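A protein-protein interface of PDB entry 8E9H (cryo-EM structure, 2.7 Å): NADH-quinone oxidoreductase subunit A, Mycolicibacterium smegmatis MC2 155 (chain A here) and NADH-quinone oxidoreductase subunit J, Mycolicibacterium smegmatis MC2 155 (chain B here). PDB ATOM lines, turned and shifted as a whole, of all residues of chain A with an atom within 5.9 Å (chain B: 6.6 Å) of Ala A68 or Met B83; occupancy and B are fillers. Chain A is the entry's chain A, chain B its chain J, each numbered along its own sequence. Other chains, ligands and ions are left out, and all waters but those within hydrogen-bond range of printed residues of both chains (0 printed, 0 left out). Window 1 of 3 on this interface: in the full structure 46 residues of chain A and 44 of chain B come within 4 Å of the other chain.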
ATOM      1  N   ILE A  62      16.623  17.998   3.855  1.00  0.00           N
ATOM      2  CA  ILE A  62      16.037  19.319   3.685  1.00  0.00           C
ATOM      3  C   ILE A  62      16.610  20.218   4.768  1.00  0.00           C
ATOM      4  O   ILE A  62      16.620  19.856   5.948  1.00  0.00           O
ATOM      5  CB  ILE A  62      14.498  19.268   3.743  1.00  0.00           C
ATOM      6  CG1 ILE A  62      14.013  18.991   5.166  1.00  0.00           C
ATOM      7  CG2 ILE A  62      13.980  18.209   2.792  1.00  0.00           C
ATOM      8  CD1 ILE A  62      12.519  18.846   5.279  1.00  0.00           C
ATOM      9  N   TYR A  64      15.508  23.045   5.785  1.00  0.00           N
ATOM     10  CA  TYR A  64      14.477  23.752   6.531  1.00  0.00           C
ATOM     11  C   TYR A  64      13.597  22.812   7.335  1.00  0.00           C
ATOM     12  O   TYR A  64      12.430  23.129   7.593  1.00  0.00           O
ATOM     13  CB  TYR A  64      13.626  24.582   5.576  1.00  0.00           C
ATOM     14  CG  TYR A  64      12.929  23.766   4.520  1.00  0.00           C
ATOM     15  CD1 TYR A  64      13.561  23.464   3.326  1.00  0.00           C
ATOM     16  CD2 TYR A  64      11.642  23.300   4.715  1.00  0.00           C
ATOM     17  CE1 TYR A  64      12.931  22.723   2.357  1.00  0.00           C
ATOM     18  CE2 TYR A  64      11.004  22.558   3.750  1.00  0.00           C
ATOM     19  CZ  TYR A  64      11.653  22.273   2.574  1.00  0.00           C
ATOM     20  OH  TYR A  64      11.022  21.531   1.606  1.00  0.00           O
ATOM     21  N   TYR A  65      14.125  21.656   7.739  1.00  0.00           N
ATOM     22  CA  TYR A  65      13.310  20.690   8.462  1.00  0.00           C
ATOM     23  C   TYR A  65      12.740  21.304   9.732  1.00  0.00           C
ATOM     24  O   TYR A  65      11.623  20.983  10.144  1.00  0.00           O
ATOM     25  CB  TYR A  65      14.134  19.449   8.796  1.00  0.00           C
ATOM     26  CG  TYR A  65      15.369  19.735   9.607  1.00  0.00           C
ATOM     27  CD1 TYR A  65      16.588  19.963   8.994  1.00  0.00           C
ATOM     28  CD2 TYR A  65      15.317  19.777  10.988  1.00  0.00           C
ATOM     29  CE1 TYR A  65      17.716  20.224   9.730  1.00  0.00           C
ATOM     30  CE2 TYR A  65      16.440  20.037  11.733  1.00  0.00           C
ATOM     31  CZ  TYR A  65      17.636  20.258  11.099  1.00  0.00           C
ATOM     32  OH  TYR A  65      18.762  20.518  11.841  1.00  0.00           O
ATOM     33  N   LEU A  66      13.502  22.185  10.375  1.00  0.00           N
ATOM     34  CA  LEU A  66      13.000  22.838  11.577  1.00  0.00           C
ATOM     35  C   LEU A  66      11.782  23.690  11.259  1.00  0.00           C
ATOM     36  O   LEU A  66      10.762  23.630  11.958  1.00  0.00           O
ATOM     37  CB  LEU A  66      14.101  23.686  12.203  1.00  0.00           C
ATOM     38  CG  LEU A  66      13.681  24.432  13.463  1.00  0.00           C
ATOM     39  CD1 LEU A  66      13.295  23.453  14.549  1.00  0.00           C
ATOM     40  CD2 LEU A  66      14.792  25.335  13.929  1.00  0.00           C
ATOM     41  N   ILE A  67      11.869  24.492  10.199  1.00  0.00           N
ATOM     42  CA  ILE A  67      10.713  25.273   9.783  1.00  0.00           C
ATOM     43  C   ILE A  67       9.588  24.345   9.362  1.00  0.00           C
ATOM     44  O   ILE A  67       8.411  24.643   9.577  1.00  0.00           O
ATOM     45  CB  ILE A  67      11.096  26.248   8.658  1.00  0.00           C
ATOM     46  CG1 ILE A  67      12.292  27.096   9.085  1.00  0.00           C
ATOM     47  CG2 ILE A  67       9.920  27.143   8.310  1.00  0.00           C
ATOM     48  CD1 ILE A  67      12.552  28.280   8.189  1.00  0.00           C
ATOM     49  N   ALA A  68       9.925  23.208   8.756  1.00  0.00           N
ATOM     50  CA  ALA A  68       8.892  22.256   8.370  1.00  0.00           C
ATOM     51  C   ALA A  68       8.125  21.760   9.587  1.00  0.00           C
ATOM     52  O   ALA A  68       6.892  21.674   9.560  1.00  0.00           O
ATOM     53  CB  ALA A  68       9.514  21.085   7.614  1.00  0.00           C
ATOM     54  N   MET A  69       8.833  21.429  10.667  1.00  0.00           N
ATOM     55  CA  MET A  69       8.155  20.988  11.879  1.00  0.00           C
ATOM     56  C   MET A  69       7.311  22.109  12.462  1.00  0.00           C
ATOM     57  O   MET A  69       6.140  21.910  12.799  1.00  0.00           O
ATOM     58  CB  MET A  69       9.169  20.501  12.911  1.00  0.00           C
ATOM     59  CG  MET A  69       9.904  19.248  12.505  1.00  0.00           C
ATOM     60  SD  MET A  69      11.035  18.672  13.777  1.00  0.00           S
ATOM     61  CE  MET A  69      12.339  19.875  13.628  1.00  0.00           C
ATOM     62  N   LEU A  70       7.890  23.302  12.585  1.00  0.00           N
ATOM     63  CA  LEU A  70       7.140  24.412  13.160  1.00  0.00           C
ATOM     64  C   LEU A  70       5.916  24.747  12.324  1.00  0.00           C
ATOM     65  O   LEU A  70       4.924  25.266  12.850  1.00  0.00           O
ATOM     66  CB  LEU A  70       8.041  25.631  13.295  1.00  0.00           C
ATOM     67  CG  LEU A  70       9.249  25.399  14.198  1.00  0.00           C
ATOM     68  CD1 LEU A  70      10.131  26.615  14.184  1.00  0.00           C
ATOM     69  CD2 LEU A  70       8.814  25.067  15.614  1.00  0.00           C
ATOM     70  N   PHE A  71       5.966  24.463  11.024  1.00  0.00           N
ATOM     71  CA  PHE A  71       4.828  24.734  10.163  1.00  0.00           C
ATOM     72  C   PHE A  71       3.610  23.949  10.609  1.00  0.00           C
ATOM     73  O   PHE A  71       2.497  24.476  10.621  1.00  0.00           O
ATOM     74  CB  PHE A  71       5.183  24.399   8.717  1.00  0.00           C
ATOM     75  CG  PHE A  71       3.999  24.320   7.806  1.00  0.00           C
ATOM     76  CD1 PHE A  71       3.489  25.457   7.214  1.00  0.00           C
ATOM     77  CD2 PHE A  71       3.402  23.107   7.532  1.00  0.00           C
ATOM     78  CE1 PHE A  71       2.402  25.385   6.372  1.00  0.00           C
ATOM     79  CE2 PHE A  71       2.315  23.031   6.691  1.00  0.00           C
ATOM     80  CZ  PHE A  71       1.817  24.171   6.112  1.00  0.00           C
ATOM     81  N   ILE A  72       3.800  22.686  10.984  1.00  0.00           N
ATOM     82  CA  ILE A  72       2.663  21.874  11.401  1.00  0.00           C
ATOM     83  C   ILE A  72       1.964  22.515  12.590  1.00  0.00           C
ATOM     84  O   ILE A  72       0.745  22.735  12.574  1.00  0.00           O
ATOM     85  CB  ILE A  72       3.126  20.444  11.730  1.00  0.00           C
ATOM     86  CG1 ILE A  72       3.767  19.791  10.505  1.00  0.00           C
ATOM     87  CG2 ILE A  72       1.959  19.616  12.217  1.00  0.00           C
ATOM     88  CD1 ILE A  72       4.549  18.545  10.829  1.00  0.00           C
ATOM     89  N   THR B  78      -3.362  18.233   5.040  1.00  0.00           N
ATOM     90  CA  THR B  78      -2.592  18.375   3.816  1.00  0.00           C
ATOM     91  C   THR B  78      -1.198  18.887   4.132  1.00  0.00           C
ATOM     92  O   THR B  78      -0.195  18.285   3.727  1.00  0.00           O
ATOM     93  CB  THR B  78      -3.314  19.324   2.863  1.00  0.00           C
ATOM     94  OG1 THR B  78      -4.639  18.839   2.624  1.00  0.00           O
ATOM     95  CG2 THR B  78      -2.584  19.428   1.545  1.00  0.00           C
ATOM     96  N   GLY B  79      -1.117  19.972   4.895  1.00  0.00           N
ATOM     97  CA  GLY B  79       0.184  20.490   5.270  1.00  0.00           C
ATOM     98  C   GLY B  79       1.020  19.479   6.029  1.00  0.00           C
ATOM     99  O   GLY B  79       2.197  19.260   5.719  1.00  0.00           O
ATOM    100  N   ALA B  80       0.409  18.841   7.025  1.00  0.00           N
ATOM    101  CA  ALA B  80       1.148  17.936   7.896  1.00  0.00           C
ATOM    102  C   ALA B  80       1.634  16.711   7.140  1.00  0.00           C
ATOM    103  O   ALA B  80       2.759  16.251   7.351  1.00  0.00           O
ATOM    104  CB  ALA B  80       0.277  17.521   9.077  1.00  0.00           C
ATOM    105  N   VAL B  81       0.799  16.156   6.263  1.00  0.00           N
ATOM    106  CA  VAL B  81       1.213  14.994   5.495  1.00  0.00           C
ATOM    107  C   VAL B  81       2.279  15.380   4.487  1.00  0.00           C
ATOM    108  O   VAL B  81       3.160  14.575   4.176  1.00  0.00           O
ATOM    109  CB  VAL B  81       0.003  14.336   4.814  1.00  0.00           C
ATOM    110  CG1 VAL B  81       0.459  13.174   3.960  1.00  0.00           C
ATOM    111  CG2 VAL B  81      -0.992  13.860   5.852  1.00  0.00           C
ATOM    112  N   MET B  82       2.238  16.604   3.959  1.00  0.00           N
ATOM    113  CA  MET B  82       3.326  17.038   3.093  1.00  0.00           C
ATOM    114  C   MET B  82       4.635  17.114   3.868  1.00  0.00           C
ATOM    115  O   MET B  82       5.691  16.702   3.372  1.00  0.00           O
ATOM    116  CB  MET B  82       2.984  18.386   2.468  1.00  0.00           C
ATOM    117  CG  MET B  82       3.996  18.868   1.456  1.00  0.00           C
ATOM    118  SD  MET B  82       3.517  20.451   0.754  1.00  0.00           S
ATOM    119  CE  MET B  82       2.142  19.948  -0.273  1.00  0.00           C
ATOM    120  N   MET B  83       4.587  17.630   5.096  1.00  0.00           N
ATOM    121  CA  MET B  83       5.789  17.652   5.924  1.00  0.00           C
ATOM    122  C   MET B  83       6.264  16.239   6.230  1.00  0.00           C
ATOM    123  O   MET B  83       7.468  15.962   6.236  1.00  0.00           O
ATOM    124  CB  MET B  83       5.533  18.421   7.217  1.00  0.00           C
ATOM    125  CG  MET B  83       5.095  19.863   7.034  1.00  0.00           C
ATOM    126  SD  MET B  83       6.133  20.833   5.922  1.00  0.00           S
ATOM    127  CE  MET B  83       5.485  20.367   4.319  1.00  0.00           C
ATOM    128  N   LEU B  84       5.331  15.331   6.507  1.00  0.00           N
ATOM    129  CA  LEU B  84       5.704  13.946   6.759  1.00  0.00           C
ATOM    130  C   LEU B  84       6.347  13.325   5.530  1.00  0.00           C
ATOM    131  O   LEU B  84       7.269  12.516   5.646  1.00  0.00           O
ATOM    132  CB  LEU B  84       4.481  13.137   7.185  1.00  0.00           C
ATOM    133  CG  LEU B  84       4.026  13.363   8.625  1.00  0.00           C
ATOM    134  CD1 LEU B  84       2.626  12.820   8.832  1.00  0.00           C
ATOM    135  CD2 LEU B  84       4.997  12.722   9.595  1.00  0.00           C
ATOM    136  N   PHE B  85       5.860  13.679   4.343  1.00  0.00           N
ATOM    137  CA  PHE B  85       6.483  13.210   3.112  1.00  0.00           C
ATOM    138  C   PHE B  85       7.906  13.740   2.995  1.00  0.00           C
ATOM    139  O   PHE B  85       8.831  13.008   2.618  1.00  0.00           O
ATOM    140  CB  PHE B  85       5.626  13.644   1.922  1.00  0.00           C
ATOM    141  CG  PHE B  85       6.370  13.731   0.628  1.00  0.00           C
ATOM    142  CD1 PHE B  85       6.455  12.635  -0.207  1.00  0.00           C
ATOM    143  CD2 PHE B  85       6.962  14.914   0.234  1.00  0.00           C
ATOM    144  CE1 PHE B  85       7.129  12.713  -1.403  1.00  0.00           C
ATOM    145  CE2 PHE B  85       7.638  14.998  -0.959  1.00  0.00           C
ATOM    146  CZ  PHE B  85       7.720  13.896  -1.780  1.00  0.00           C
ATOM    147  N   LEU B  86       8.102  15.015   3.332  1.00  0.00           N
ATOM    148  CA  LEU B  86       9.451  15.567   3.335  1.00  0.00           C
ATOM    149  C   LEU B  86      10.356  14.790   4.277  1.00  0.00           C
ATOM    150  O   LEU B  86      11.497  14.463   3.932  1.00  0.00           O
ATOM    151  CB  LEU B  86       9.425  17.038   3.741  1.00  0.00           C
ATOM    152  CG  LEU B  86       8.929  18.034   2.702  1.00  0.00           C
ATOM    153  CD1 LEU B  86       8.745  19.390   3.348  1.00  0.00           C
ATOM    154  CD2 LEU B  86       9.900  18.113   1.545  1.00  0.00           C
ATOM    155  N   PHE B  87       9.865  14.485   5.473  1.00  0.00           N
ATOM    156  CA  PHE B  87      10.685  13.763   6.436  1.00  0.00           C
ATOM    157  C   PHE B  87      10.902  12.318   6.017  1.00  0.00           C
ATOM    158  O   PHE B  87      11.929  11.725   6.356  1.00  0.00           O
ATOM    159  CB  PHE B  87      10.049  13.844   7.817  1.00  0.00           C
ATOM    160  CG  PHE B  87      10.372  15.109   8.541  1.00  0.00           C
ATOM    161  CD1 PHE B  87      11.583  15.258   9.181  1.00  0.00           C
ATOM    162  CD2 PHE B  87       9.483  16.165   8.545  1.00  0.00           C
ATOM    163  CE1 PHE B  87      11.891  16.425   9.836  1.00  0.00           C
ATOM    164  CE2 PHE B  87       9.789  17.333   9.196  1.00  0.00           C
ATOM    165  CZ  PHE B  87      10.994  17.463   9.841  1.00  0.00           C
ATOM    166  N   VAL B  88       9.957  11.736   5.284  1.00  0.00           N
ATOM    167  CA  VAL B  88      10.167  10.409   4.718  1.00  0.00           C
ATOM    168  C   VAL B  88      11.323  10.445   3.732  1.00  0.00           C
ATOM    169  O   VAL B  88      12.191   9.566   3.727  1.00  0.00           O
ATOM    170  CB  VAL B  88       8.877   9.901   4.052  1.00  0.00           C
ATOM    171  CG1 VAL B  88       9.181   8.764   3.102  1.00  0.00           C
ATOM    172  CG2 VAL B  88       7.883   9.458   5.101  1.00  0.00           C
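Among the printed residues, merely in contact across the chains: Met A69 with Phe B87 (3.4 Å), Tyr A64 with Leu B86 (3.6 Å), Tyr A65 with Phe B87 (3.6 Å), Ala A68 with Met B83 (3.6 Å), Phe A71 with Gly B79 (3.6 Å), Phe A71 with Met B83 (3.7 Å), Ile A72 with Met B83 (3.7 Å) and Ile A62 with Leu B86 (3.9 Å).
Of chain B, only Met B83 (3.6 Å) comes within 4 Å of Ala A68. Of chain A, only Ala A68 (3.6 Å), Phe A71 (3.7 Å) and Ile A72 (3.7 Å) come within 4 Å of Met B83. Of the printed residues of chain B, Met A69 touches Phe B87. Of the printed residues of chain B, Tyr A64 touches Leu B86. Val B81 touches none of the printed residues of chain A. The nearest residue of chain B that does not touch Ala A68 is Phe B87 (4.1 Å). The nearest printed residue of chain B that does not touch Ile A72 is Ala B80 (4.1 Å).
Of the 11 printed residues of chain B, 4 touch a printed residue of chain A. Hydrophobic or aromatic side chains of chain B that line the printed part of chain A: Met B83, Leu B86 and Phe B87. Along chain B the printed residues that touch a printed residue of chain A span positions 79 to 87. Of the 10 printed residues of chain A, 7 touch a printed residue of chain B. Printed residues of chain A that touch a printed residue of chain B: Ile A62, Tyr A64, Tyr A65, Ala A68, Met A69, Phe A71 and Ile A72. Hydrophobic or aromatic side chains of chain A within 4 Å of the printed part of chain B: Ile A62, Tyr A64, Tyr A65, Ala A68, Met A69, Phe A71 and Ile A72. Among the printed residues, 8 pairs touch across the chains. Among the printed residues, no Asp or Glu carboxylate lies within 4 Å of a Lys or Arg side-chain nitrogen of the other chain.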
